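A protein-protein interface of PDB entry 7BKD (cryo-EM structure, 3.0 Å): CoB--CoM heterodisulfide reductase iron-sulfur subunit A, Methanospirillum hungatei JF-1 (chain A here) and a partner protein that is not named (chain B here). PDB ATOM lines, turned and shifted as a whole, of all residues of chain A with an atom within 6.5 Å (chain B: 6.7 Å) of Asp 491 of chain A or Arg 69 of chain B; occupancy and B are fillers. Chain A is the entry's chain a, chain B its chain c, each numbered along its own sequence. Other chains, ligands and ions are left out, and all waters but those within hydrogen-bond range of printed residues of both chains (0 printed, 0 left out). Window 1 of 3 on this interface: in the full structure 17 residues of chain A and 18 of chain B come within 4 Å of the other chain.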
ATOM      1  N   TYR A 444      -5.068   1.952 -27.931  1.00  0.00           N
ATOM      2  CA  TYR A 444      -3.676   1.573 -27.815  1.00  0.00           C
ATOM      3  C   TYR A 444      -3.307   1.304 -26.367  1.00  0.00           C
ATOM      4  O   TYR A 444      -4.079   1.531 -25.434  1.00  0.00           O
ATOM      5  CB  TYR A 444      -2.759   2.660 -28.392  1.00  0.00           C
ATOM      6  CG  TYR A 444      -2.521   3.826 -27.458  1.00  0.00           C
ATOM      7  CD1 TYR A 444      -3.366   4.925 -27.462  1.00  0.00           C
ATOM      8  CD2 TYR A 444      -1.451   3.827 -26.574  1.00  0.00           C
ATOM      9  CE1 TYR A 444      -3.153   5.988 -26.614  1.00  0.00           C
ATOM     10  CE2 TYR A 444      -1.232   4.881 -25.726  1.00  0.00           C
ATOM     11  CZ  TYR A 444      -2.084   5.961 -25.750  1.00  0.00           C
ATOM     12  OH  TYR A 444      -1.862   7.017 -24.897  1.00  0.00           O
ATOM     13  N   LYS A 467      -7.206  10.143 -33.135  1.00  0.00           N
ATOM     14  CA  LYS A 467      -7.572  10.094 -31.727  1.00  0.00           C
ATOM     15  C   LYS A 467      -6.923   8.883 -31.074  1.00  0.00           C
ATOM     16  O   LYS A 467      -6.983   7.774 -31.611  1.00  0.00           O
ATOM     17  CB  LYS A 467      -9.091  10.036 -31.572  1.00  0.00           C
ATOM     18  CG  LYS A 467      -9.856  11.227 -32.154  1.00  0.00           C
ATOM     19  CD  LYS A 467      -9.657  12.512 -31.351  1.00  0.00           C
ATOM     20  CE  LYS A 467      -8.528  13.379 -31.891  1.00  0.00           C
ATOM     21  NZ  LYS A 467      -8.426  14.671 -31.158  1.00  0.00           N
ATOM     22  N   PHE A 468      -6.299   9.096 -29.921  1.00  0.00           N
ATOM     23  CA  PHE A 468      -5.591   8.038 -29.212  1.00  0.00           C
ATOM     24  C   PHE A 468      -6.278   7.798 -27.876  1.00  0.00           C
ATOM     25  O   PHE A 468      -6.173   8.621 -26.962  1.00  0.00           O
ATOM     26  CB  PHE A 468      -4.119   8.390 -29.010  1.00  0.00           C
ATOM     27  CG  PHE A 468      -3.313   8.372 -30.273  1.00  0.00           C
ATOM     28  CD1 PHE A 468      -3.479   9.360 -31.228  1.00  0.00           C
ATOM     29  CD2 PHE A 468      -2.415   7.350 -30.521  1.00  0.00           C
ATOM     30  CE1 PHE A 468      -2.745   9.348 -32.391  1.00  0.00           C
ATOM     31  CE2 PHE A 468      -1.683   7.326 -31.688  1.00  0.00           C
ATOM     32  CZ  PHE A 468      -1.848   8.329 -32.624  1.00  0.00           C
ATOM     33  N   ILE A 469      -6.971   6.671 -27.761  1.00  0.00           N
ATOM     34  CA  ILE A 469      -7.600   6.252 -26.516  1.00  0.00           C
ATOM     35  C   ILE A 469      -6.699   5.200 -25.888  1.00  0.00           C
ATOM     36  O   ILE A 469      -6.528   4.107 -26.439  1.00  0.00           O
ATOM     37  CB  ILE A 469      -9.019   5.714 -26.742  1.00  0.00           C
ATOM     38  CG1 ILE A 469      -9.944   6.815 -27.264  1.00  0.00           C
ATOM     39  CG2 ILE A 469      -9.577   5.116 -25.463  1.00  0.00           C
ATOM     40  CD1 ILE A 469     -10.006   6.915 -28.766  1.00  0.00           C
ATOM     41  N   ARG A 470      -6.121   5.522 -24.737  1.00  0.00           N
ATOM     42  CA  ARG A 470      -5.220   4.606 -24.042  1.00  0.00           C
ATOM     43  C   ARG A 470      -6.061   3.605 -23.262  1.00  0.00           C
ATOM     44  O   ARG A 470      -6.349   3.784 -22.079  1.00  0.00           O
ATOM     45  CB  ARG A 470      -4.267   5.368 -23.134  1.00  0.00           C
ATOM     46  CG  ARG A 470      -3.011   4.604 -22.778  1.00  0.00           C
ATOM     47  CD  ARG A 470      -3.094   4.069 -21.385  1.00  0.00           C
ATOM     48  NE  ARG A 470      -1.896   3.353 -20.977  1.00  0.00           N
ATOM     49  CZ  ARG A 470      -1.880   2.460 -19.995  1.00  0.00           C
ATOM     50  NH1 ARG A 470      -2.999   2.183 -19.344  1.00  0.00           N
ATOM     51  NH2 ARG A 470      -0.758   1.838 -19.669  1.00  0.00           N
ATOM     52  N   GLY A 471      -6.460   2.538 -23.943  1.00  0.00           N
ATOM     53  CA  GLY A 471      -7.179   1.453 -23.315  1.00  0.00           C
ATOM     54  C   GLY A 471      -7.294   0.236 -24.207  1.00  0.00           C
ATOM     55  O   GLY A 471      -7.679   0.345 -25.374  1.00  0.00           O
ATOM     56  N   THR A 489     -14.401  -0.326 -24.148  1.00  0.00           N
ATOM     57  CA  THR A 489     -13.151  -0.373 -23.400  1.00  0.00           C
ATOM     58  C   THR A 489     -13.202   0.712 -22.331  1.00  0.00           C
ATOM     59  O   THR A 489     -14.257   1.289 -22.062  1.00  0.00           O
ATOM     60  CB  THR A 489     -11.938  -0.211 -24.325  1.00  0.00           C
ATOM     61  OG1 THR A 489     -10.737  -0.197 -23.545  1.00  0.00           O
ATOM     62  CG2 THR A 489     -12.033   1.076 -25.126  1.00  0.00           C
ATOM     63  N   GLU A 490     -12.067   0.970 -21.698  1.00  0.00           N
ATOM     64  CA  GLU A 490     -11.888   2.145 -20.867  1.00  0.00           C
ATOM     65  C   GLU A 490     -10.892   3.067 -21.551  1.00  0.00           C
ATOM     66  O   GLU A 490      -9.946   2.606 -22.194  1.00  0.00           O
ATOM     67  CB  GLU A 490     -11.339   1.806 -19.479  1.00  0.00           C
ATOM     68  CG  GLU A 490     -11.249   3.027 -18.568  1.00  0.00           C
ATOM     69  CD  GLU A 490     -10.668   2.727 -17.205  1.00  0.00           C
ATOM     70  OE1 GLU A 490     -10.266   1.574 -16.970  1.00  0.00           O
ATOM     71  OE2 GLU A 490     -10.627   3.645 -16.360  1.00  0.00           O
ATOM     72  N   ASP A 491     -11.097   4.367 -21.413  1.00  0.00           N
ATOM     73  CA  ASP A 491     -10.034   5.321 -21.684  1.00  0.00           C
ATOM     74  C   ASP A 491      -9.444   5.542 -20.294  1.00  0.00           C
ATOM     75  O   ASP A 491     -10.032   6.241 -19.462  1.00  0.00           O
ATOM     76  CB  ASP A 491     -10.569   6.599 -22.323  1.00  0.00           C
ATOM     77  CG  ASP A 491      -9.469   7.575 -22.715  1.00  0.00           C
ATOM     78  OD1 ASP A 491      -8.298   7.376 -22.325  1.00  0.00           O
ATOM     79  OD2 ASP A 491      -9.786   8.556 -23.419  1.00  0.00           O
ATOM     80  N   THR A 492      -8.323   4.864 -20.021  1.00  0.00           N
ATOM     81  CA  THR A 492      -7.742   4.870 -18.680  1.00  0.00           C
ATOM     82  C   THR A 492      -7.269   6.261 -18.294  1.00  0.00           C
ATOM     83  O   THR A 492      -7.435   6.686 -17.146  1.00  0.00           O
ATOM     84  CB  THR A 492      -6.584   3.877 -18.599  1.00  0.00           C
ATOM     85  OG1 THR A 492      -5.512   4.333 -19.428  1.00  0.00           O
ATOM     86  CG2 THR A 492      -7.025   2.498 -19.062  1.00  0.00           C
ATOM     87  N   LEU A 493      -6.644   6.961 -19.227  1.00  0.00           N
ATOM     88  CA  LEU A 493      -6.514   8.402 -19.114  1.00  0.00           C
ATOM     89  C   LEU A 493      -7.905   8.994 -19.278  1.00  0.00           C
ATOM     90  O   LEU A 493      -8.697   8.497 -20.075  1.00  0.00           O
ATOM     91  CB  LEU A 493      -5.562   8.905 -20.192  1.00  0.00           C
ATOM     92  CG  LEU A 493      -4.156   8.354 -19.941  1.00  0.00           C
ATOM     93  CD1 LEU A 493      -3.212   8.708 -21.063  1.00  0.00           C
ATOM     94  CD2 LEU A 493      -3.620   8.825 -18.610  1.00  0.00           C
ATOM     95  N   LEU A 494      -8.226  10.014 -18.481  1.00  0.00           N
ATOM     96  CA  LEU A 494      -9.599  10.506 -18.325  1.00  0.00           C
ATOM     97  C   LEU A 494     -10.426   9.539 -17.482  1.00  0.00           C
ATOM     98  O   LEU A 494     -11.517   9.890 -17.027  1.00  0.00           O
ATOM     99  CB  LEU A 494     -10.285  10.720 -19.682  1.00  0.00           C
ATOM    100  CG  LEU A 494     -11.690  11.313 -19.794  1.00  0.00           C
ATOM    101  CD1 LEU A 494     -11.709  12.782 -19.402  1.00  0.00           C
ATOM    102  CD2 LEU A 494     -12.261  11.093 -21.185  1.00  0.00           C
ATOM    103  N   GLY A 495      -9.888   8.346 -17.231  1.00  0.00           N
ATOM    104  CA  GLY A 495     -10.510   7.322 -16.412  1.00  0.00           C
ATOM    105  C   GLY A 495     -12.001   7.107 -16.581  1.00  0.00           C
ATOM    106  O   GLY A 495     -12.749   7.223 -15.607  1.00  0.00           O
ATOM    107  N   ARG A 496     -12.459   6.795 -17.788  1.00  0.00           N
ATOM    108  CA  ARG A 496     -13.889   6.582 -17.967  1.00  0.00           C
ATOM    109  C   ARG A 496     -14.140   5.432 -18.927  1.00  0.00           C
ATOM    110  O   ARG A 496     -13.373   5.231 -19.874  1.00  0.00           O
ATOM    111  CB  ARG A 496     -14.594   7.841 -18.494  1.00  0.00           C
ATOM    112  CG  ARG A 496     -15.099   8.779 -17.412  1.00  0.00           C
ATOM    113  CD  ARG A 496     -15.427  10.151 -17.979  1.00  0.00           C
ATOM    114  NE  ARG A 496     -16.590  10.100 -18.855  1.00  0.00           N
ATOM    115  CZ  ARG A 496     -16.961  11.083 -19.667  1.00  0.00           C
ATOM    116  NH1 ARG A 496     -16.257  12.204 -19.721  1.00  0.00           N
ATOM    117  NH2 ARG A 496     -18.034  10.942 -20.428  1.00  0.00           N
ATOM    118  N   PRO A 497     -15.215   4.674 -18.720  1.00  0.00           N
ATOM    119  CA  PRO A 497     -15.625   3.695 -19.731  1.00  0.00           C
ATOM    120  C   PRO A 497     -15.994   4.390 -21.032  1.00  0.00           C
ATOM    121  O   PRO A 497     -16.437   5.538 -21.043  1.00  0.00           O
ATOM    122  CB  PRO A 497     -16.837   3.005 -19.094  1.00  0.00           C
ATOM    123  CG  PRO A 497     -17.285   3.928 -18.014  1.00  0.00           C
ATOM    124  CD  PRO A 497     -16.053   4.599 -17.514  1.00  0.00           C
ATOM    125  N   VAL A 498     -15.785   3.684 -22.140  1.00  0.00           N
ATOM    126  CA  VAL A 498     -15.913   4.241 -23.480  1.00  0.00           C
ATOM    127  C   VAL A 498     -16.610   3.221 -24.371  1.00  0.00           C
ATOM    128  O   VAL A 498     -16.258   2.035 -24.363  1.00  0.00           O
ATOM    129  CB  VAL A 498     -14.539   4.617 -24.075  1.00  0.00           C
ATOM    130  CG1 VAL A 498     -14.698   5.185 -25.457  1.00  0.00           C
ATOM    131  CG2 VAL A 498     -13.823   5.609 -23.190  1.00  0.00           C
ATOM    132  N   TYR B  20     -18.080   7.635 -22.318  1.00  0.00           N
ATOM    133  CA  TYR B  20     -17.825   8.573 -23.401  1.00  0.00           C
ATOM    134  C   TYR B  20     -18.345   7.988 -24.707  1.00  0.00           C
ATOM    135  O   TYR B  20     -18.040   6.842 -25.049  1.00  0.00           O
ATOM    136  CB  TYR B  20     -16.333   8.878 -23.507  1.00  0.00           C
ATOM    137  CG  TYR B  20     -15.956   9.610 -24.776  1.00  0.00           C
ATOM    138  CD1 TYR B  20     -16.114  10.984 -24.878  1.00  0.00           C
ATOM    139  CD2 TYR B  20     -15.452   8.926 -25.874  1.00  0.00           C
ATOM    140  CE1 TYR B  20     -15.778  11.655 -26.034  1.00  0.00           C
ATOM    141  CE2 TYR B  20     -15.115   9.589 -27.036  1.00  0.00           C
ATOM    142  CZ  TYR B  20     -15.279  10.954 -27.109  1.00  0.00           C
ATOM    143  OH  TYR B  20     -14.942  11.623 -28.262  1.00  0.00           O
ATOM    144  N   CYS B  44      -1.184  17.177 -27.056  1.00  0.00           N
ATOM    145  CA  CYS B  44      -0.931  16.580 -25.756  1.00  0.00           C
ATOM    146  C   CYS B  44      -0.987  15.061 -25.852  1.00  0.00           C
ATOM    147  O   CYS B  44      -1.884  14.496 -26.479  1.00  0.00           O
ATOM    148  CB  CYS B  44      -1.951  17.090 -24.738  1.00  0.00           C
ATOM    149  SG  CYS B  44      -1.900  16.311 -23.120  1.00  0.00           S
ATOM    150  N   GLN B  46      -0.489  13.361 -22.744  1.00  0.00           N
ATOM    151  CA  GLN B  46      -0.917  12.973 -21.399  1.00  0.00           C
ATOM    152  C   GLN B  46       0.223  12.382 -20.574  1.00  0.00           C
ATOM    153  O   GLN B  46       0.083  11.338 -19.939  1.00  0.00           O
ATOM    154  CB  GLN B  46      -2.100  12.004 -21.471  1.00  0.00           C
ATOM    155  CG  GLN B  46      -3.312  12.561 -22.195  1.00  0.00           C
ATOM    156  CD  GLN B  46      -4.175  13.421 -21.299  1.00  0.00           C
ATOM    157  OE1 GLN B  46      -4.676  12.961 -20.278  1.00  0.00           O
ATOM    158  NE2 GLN B  46      -4.348  14.680 -21.674  1.00  0.00           N
ATOM    159  N   ILE B  64      -5.135  19.668 -14.360  1.00  0.00           N
ATOM    160  CA  ILE B  64      -4.981  20.351 -15.641  1.00  0.00           C
ATOM    161  C   ILE B  64      -4.903  19.341 -16.784  1.00  0.00           C
ATOM    162  O   ILE B  64      -5.374  19.604 -17.897  1.00  0.00           O
ATOM    163  CB  ILE B  64      -3.757  21.290 -15.590  1.00  0.00           C
ATOM    164  CG1 ILE B  64      -3.499  21.936 -16.949  1.00  0.00           C
ATOM    165  CG2 ILE B  64      -2.522  20.566 -15.087  1.00  0.00           C
ATOM    166  CD1 ILE B  64      -4.650  22.732 -17.464  1.00  0.00           C
ATOM    167  N   ARG B  65      -4.326  18.165 -16.525  1.00  0.00           N
ATOM    168  CA  ARG B  65      -4.231  17.140 -17.560  1.00  0.00           C
ATOM    169  C   ARG B  65      -5.609  16.659 -18.003  1.00  0.00           C
ATOM    170  O   ARG B  65      -5.835  16.415 -19.193  1.00  0.00           O
ATOM    171  CB  ARG B  65      -3.383  15.970 -17.064  1.00  0.00           C
ATOM    172  CG  ARG B  65      -3.233  14.844 -18.065  1.00  0.00           C
ATOM    173  CD  ARG B  65      -2.449  13.683 -17.487  1.00  0.00           C
ATOM    174  NE  ARG B  65      -3.101  13.100 -16.317  1.00  0.00           N
ATOM    175  CZ  ARG B  65      -4.166  12.308 -16.370  1.00  0.00           C
ATOM    176  NH1 ARG B  65      -4.708  11.996 -17.537  1.00  0.00           N
ATOM    177  NH2 ARG B  65      -4.688  11.826 -15.254  1.00  0.00           N
ATOM    178  N   LEU B  66      -6.548  16.515 -17.062  1.00  0.00           N
ATOM    179  CA  LEU B  66      -7.910  16.157 -17.446  1.00  0.00           C
ATOM    180  C   LEU B  66      -8.545  17.234 -18.312  1.00  0.00           C
ATOM    181  O   LEU B  66      -9.287  16.926 -19.247  1.00  0.00           O
ATOM    182  CB  LEU B  66      -8.776  15.888 -16.215  1.00  0.00           C
ATOM    183  CG  LEU B  66      -8.440  14.684 -15.343  1.00  0.00           C
ATOM    184  CD1 LEU B  66      -9.325  14.674 -14.109  1.00  0.00           C
ATOM    185  CD2 LEU B  66      -8.605  13.400 -16.139  1.00  0.00           C
ATOM    186  N   PHE B  67      -8.278  18.505 -18.010  1.00  0.00           N
ATOM    187  CA  PHE B  67      -8.799  19.578 -18.851  1.00  0.00           C
ATOM    188  C   PHE B  67      -8.204  19.522 -20.253  1.00  0.00           C
ATOM    189  O   PHE B  67      -8.908  19.755 -21.242  1.00  0.00           O
ATOM    190  CB  PHE B  67      -8.533  20.934 -18.201  1.00  0.00           C
ATOM    191  CG  PHE B  67      -9.583  21.336 -17.216  1.00  0.00           C
ATOM    192  CD1 PHE B  67     -10.831  21.757 -17.647  1.00  0.00           C
ATOM    193  CD2 PHE B  67      -9.334  21.281 -15.859  1.00  0.00           C
ATOM    194  CE1 PHE B  67     -11.802  22.121 -16.744  1.00  0.00           C
ATOM    195  CE2 PHE B  67     -10.301  21.642 -14.953  1.00  0.00           C
ATOM    196  CZ  PHE B  67     -11.537  22.066 -15.394  1.00  0.00           C
ATOM    197  N   MET B  68      -6.910  19.212 -20.358  1.00  0.00           N
ATOM    198  CA  MET B  68      -6.302  19.056 -21.676  1.00  0.00           C
ATOM    199  C   MET B  68      -6.931  17.895 -22.435  1.00  0.00           C
ATOM    200  O   MET B  68      -7.190  17.995 -23.641  1.00  0.00           O
ATOM    201  CB  MET B  68      -4.793  18.859 -21.540  1.00  0.00           C
ATOM    202  CG  MET B  68      -4.066  20.068 -20.969  1.00  0.00           C
ATOM    203  SD  MET B  68      -4.119  21.519 -22.034  1.00  0.00           S
ATOM    204  CE  MET B  68      -3.738  20.806 -23.629  1.00  0.00           C
ATOM    205  N   ARG B  69      -7.187  16.786 -21.740  1.00  0.00           N
ATOM    206  CA  ARG B  69      -7.846  15.644 -22.366  1.00  0.00           C
ATOM    207  C   ARG B  69      -9.245  16.007 -22.844  1.00  0.00           C
ATOM    208  O   ARG B  69      -9.656  15.616 -23.942  1.00  0.00           O
ATOM    209  CB  ARG B  69      -7.899  14.476 -21.384  1.00  0.00           C
ATOM    210  CG  ARG B  69      -8.324  13.161 -21.999  1.00  0.00           C
ATOM    211  CD  ARG B  69      -7.246  12.596 -22.895  1.00  0.00           C
ATOM    212  NE  ARG B  69      -7.714  11.425 -23.624  1.00  0.00           N
ATOM    213  CZ  ARG B  69      -7.534  11.234 -24.924  1.00  0.00           C
ATOM    214  NH1 ARG B  69      -6.891  12.140 -25.645  1.00  0.00           N
ATOM    215  NH2 ARG B  69      -7.998  10.136 -25.503  1.00  0.00           N
ATOM    216  N   ARG B  70      -9.991  16.753 -22.028  1.00  0.00           N
ATOM    217  CA  ARG B  70     -11.329  17.188 -22.412  1.00  0.00           C
ATOM    218  C   ARG B  70     -11.282  18.101 -23.628  1.00  0.00           C
ATOM    219  O   ARG B  70     -12.147  18.023 -24.507  1.00  0.00           O
ATOM    220  CB  ARG B  70     -11.999  17.896 -21.240  1.00  0.00           C
ATOM    221  CG  ARG B  70     -12.439  16.974 -20.128  1.00  0.00           C
ATOM    222  CD  ARG B  70     -12.807  17.759 -18.894  1.00  0.00           C
ATOM    223  NE  ARG B  70     -13.229  16.888 -17.806  1.00  0.00           N
ATOM    224  CZ  ARG B  70     -13.496  17.308 -16.576  1.00  0.00           C
ATOM    225  NH1 ARG B  70     -13.376  18.592 -16.273  1.00  0.00           N
ATOM    226  NH2 ARG B  70     -13.876  16.444 -15.647  1.00  0.00           N
ATOM    227  N   CYS B  71     -10.286  18.984 -23.685  1.00  0.00           N
ATOM    228  CA  CYS B  71     -10.122  19.835 -24.857  1.00  0.00           C
ATOM    229  C   CYS B  71      -9.837  19.010 -26.107  1.00  0.00           C
ATOM    230  O   CYS B  71     -10.422  19.256 -27.167  1.00  0.00           O
ATOM    231  CB  CYS B  71      -9.002  20.846 -24.618  1.00  0.00           C
ATOM    232  SG  CYS B  71      -8.415  21.658 -26.113  1.00  0.00           S
ATOM    233  N   VAL B  72      -8.946  18.023 -25.998  1.00  0.00           N
ATOM    234  CA  VAL B  72      -8.628  17.179 -27.150  1.00  0.00           C
ATOM    235  C   VAL B  72      -9.857  16.405 -27.607  1.00  0.00           C
ATOM    236  O   VAL B  72     -10.133  16.305 -28.809  1.00  0.00           O
ATOM    237  CB  VAL B  72      -7.452  16.240 -26.821  1.00  0.00           C
ATOM    238  CG1 VAL B  72      -7.193  15.289 -27.972  1.00  0.00           C
ATOM    239  CG2 VAL B  72      -6.206  17.053 -26.540  1.00  0.00           C
ATOM    240  N   LEU B  73     -10.619  15.855 -26.665  1.00  0.00           N
ATOM    241  CA  LEU B  73     -11.821  15.102 -26.998  1.00  0.00           C
ATOM    242  C   LEU B  73     -13.043  15.988 -27.189  1.00  0.00           C
ATOM    243  O   LEU B  73     -14.129  15.462 -27.452  1.00  0.00           O
ATOM    244  CB  LEU B  73     -12.106  14.059 -25.917  1.00  0.00           C
ATOM    245  CG  LEU B  73     -11.034  12.980 -25.772  1.00  0.00           C
ATOM    246  CD1 LEU B  73     -11.249  12.172 -24.512  1.00  0.00           C
ATOM    247  CD2 LEU B  73     -11.021  12.080 -26.995  1.00  0.00           C
ATOM    248  N   GLY B  74     -12.899  17.302 -27.055  1.00  0.00           N
ATOM    249  CA  GLY B  74     -14.007  18.210 -27.308  1.00  0.00           C
ATOM    250  C   GLY B  74     -15.186  18.016 -26.381  1.00  0.00           C
ATOM    251  O   GLY B  74     -16.335  18.001 -26.837  1.00  0.00           O
ATOM    252  N   LEU B  75     -14.928  17.865 -25.087  1.00  0.00           N
ATOM    253  CA  LEU B  75     -15.990  17.606 -24.119  1.00  0.00           C
ATOM    254  C   LEU B  75     -16.417  18.909 -23.447  1.00  0.00           C
ATOM    255  O   LEU B  75     -16.116  19.183 -22.286  1.00  0.00           O
ATOM    256  CB  LEU B  75     -15.532  16.571 -23.099  1.00  0.00           C
ATOM    257  CG  LEU B  75     -15.365  15.157 -23.654  1.00  0.00           C
ATOM    258  CD1 LEU B  75     -14.788  14.236 -22.604  1.00  0.00           C
ATOM    259  CD2 LEU B  75     -16.696  14.640 -24.151  1.00  0.00           C
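O of Arg 70 of chain B sits at hydrogen-bond distance from N of Leu 75 of chain B, 2.8 Å away.
OD1 of Asp 491 of chain A lies close to O of Leu 493 of chain A (2.5 Å).
The backbone NH (N) of Asp 491 of chain A sits at hydrogen-bond distance from the backbone carbonyl oxygen (O) of Arg 496 of chain A (2.9 Å).
The side-chain sulfur (SG) of Cys 44 of chain B lies close to the side-chain amide nitrogen (NE2) of Gln 46 of chain B (3.3 Å).
OE1 of Gln 46 of chain B lies within hydrogen-bond range of NH1 of Arg 65 of chain B.
The backbone NH (N) of Val 498 of chain A is in hydrogen-bond range of the backbone carbonyl oxygen (O) of Thr 489 of chain A, 2.8 Å away.
CD1 of Leu 493 of chain A touches CB of Gln 46 of chain B, 3.5 Å away.
Leu 493 of chain A touches Arg 65 of chain B (CD2 to NH1, 3.5 Å).
Leu 494 of chain A touches Leu 66 of chain B (CA to CD2, 3.8 Å).
CG of Arg 69 of chain B touches CB of Leu 494 of chain A, 3.9 Å away.
Leu 494 of chain A touches Leu 73 of chain B.
NH2 of Arg 496 of chain A touches CA of Tyr 20 of chain B, at 3.8 Å.
Leu 75 of chain B touches Arg 496 of chain A (CD1 to NH1, 3.8 Å).
Tyr 20 of chain B touches Val 498 of chain A.
Of the printed residues of chain B, Phe 468 of chain A touches Arg 69.
Asp 491 of chain A touches one residue of chain B.
Printed residues of chain B within 4 Å of Arg 496 of chain A: Tyr 20 (3.8 Å) and Leu 75 (3.8 Å).
Printed residues of chain A within 4 Å of Gln 46 of chain B: Leu 493 (3.5 Å).
Of the printed residues of chain A, Arg 65 of chain B touches Leu 493.
Arg 69 of chain B touches just these residues of chain A: Phe 468, Asp 491 and Leu 494.
Arg 70 of chain B touches none of the printed residues of chain A.
Of the printed residues of chain A, Leu 75 of chain B touches Arg 496.
The nearest residue of chain B that does not touch Asp 491 of chain A is Leu 73 of chain B (4.1 Å).
The nearest printed residue of chain B that does not touch Val 498 of chain A is Leu 73 of chain B (7.2 Å).
Printed residues of chain B that touch a printed residue of chain A: Tyr 20, Gln 46, Arg 65, Leu 66, Arg 69, Val 72, Leu 73 and Leu 75.
Hydrophobic or aromatic side chains of chain B within 4 Å of the printed part of chain A: Tyr 20, Leu 66, Val 72, Leu 73 and Leu 75.
Of the 16 printed residues of chain A, 8 touch a printed residue of chain B.
Printed residues of chain A that touch a printed residue of chain B: Lys 467, Phe 468, Asp 491, Leu 493, Leu 494, Arg 496, Pro 497 and Val 498.
Hydrophobic or aromatic side chains of chain A that line the printed part of chain B: Leu 493, Leu 494 and Val 498.
Among the printed residues, 12 pairs touch across the chains.
NZ of Lys 467 of chain A lies within hydrogen-bond range of O of Val 72 of chain B.
N of Tyr 20 of chain B is in hydrogen-bond range of O of Pro 497 of chain A, 3.0 Å away.
NH2 of Arg 69 of chain B lies within salt-bridge range of OD2 of Asp 491 of chain A, 3.2 Å away.
The backbone carbonyl oxygen (O) of Phe 468 of chain A lies within hydrogen-bond range of the guanidinium group (NH2) of Arg 69 of chain B, 2.8 Å away.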
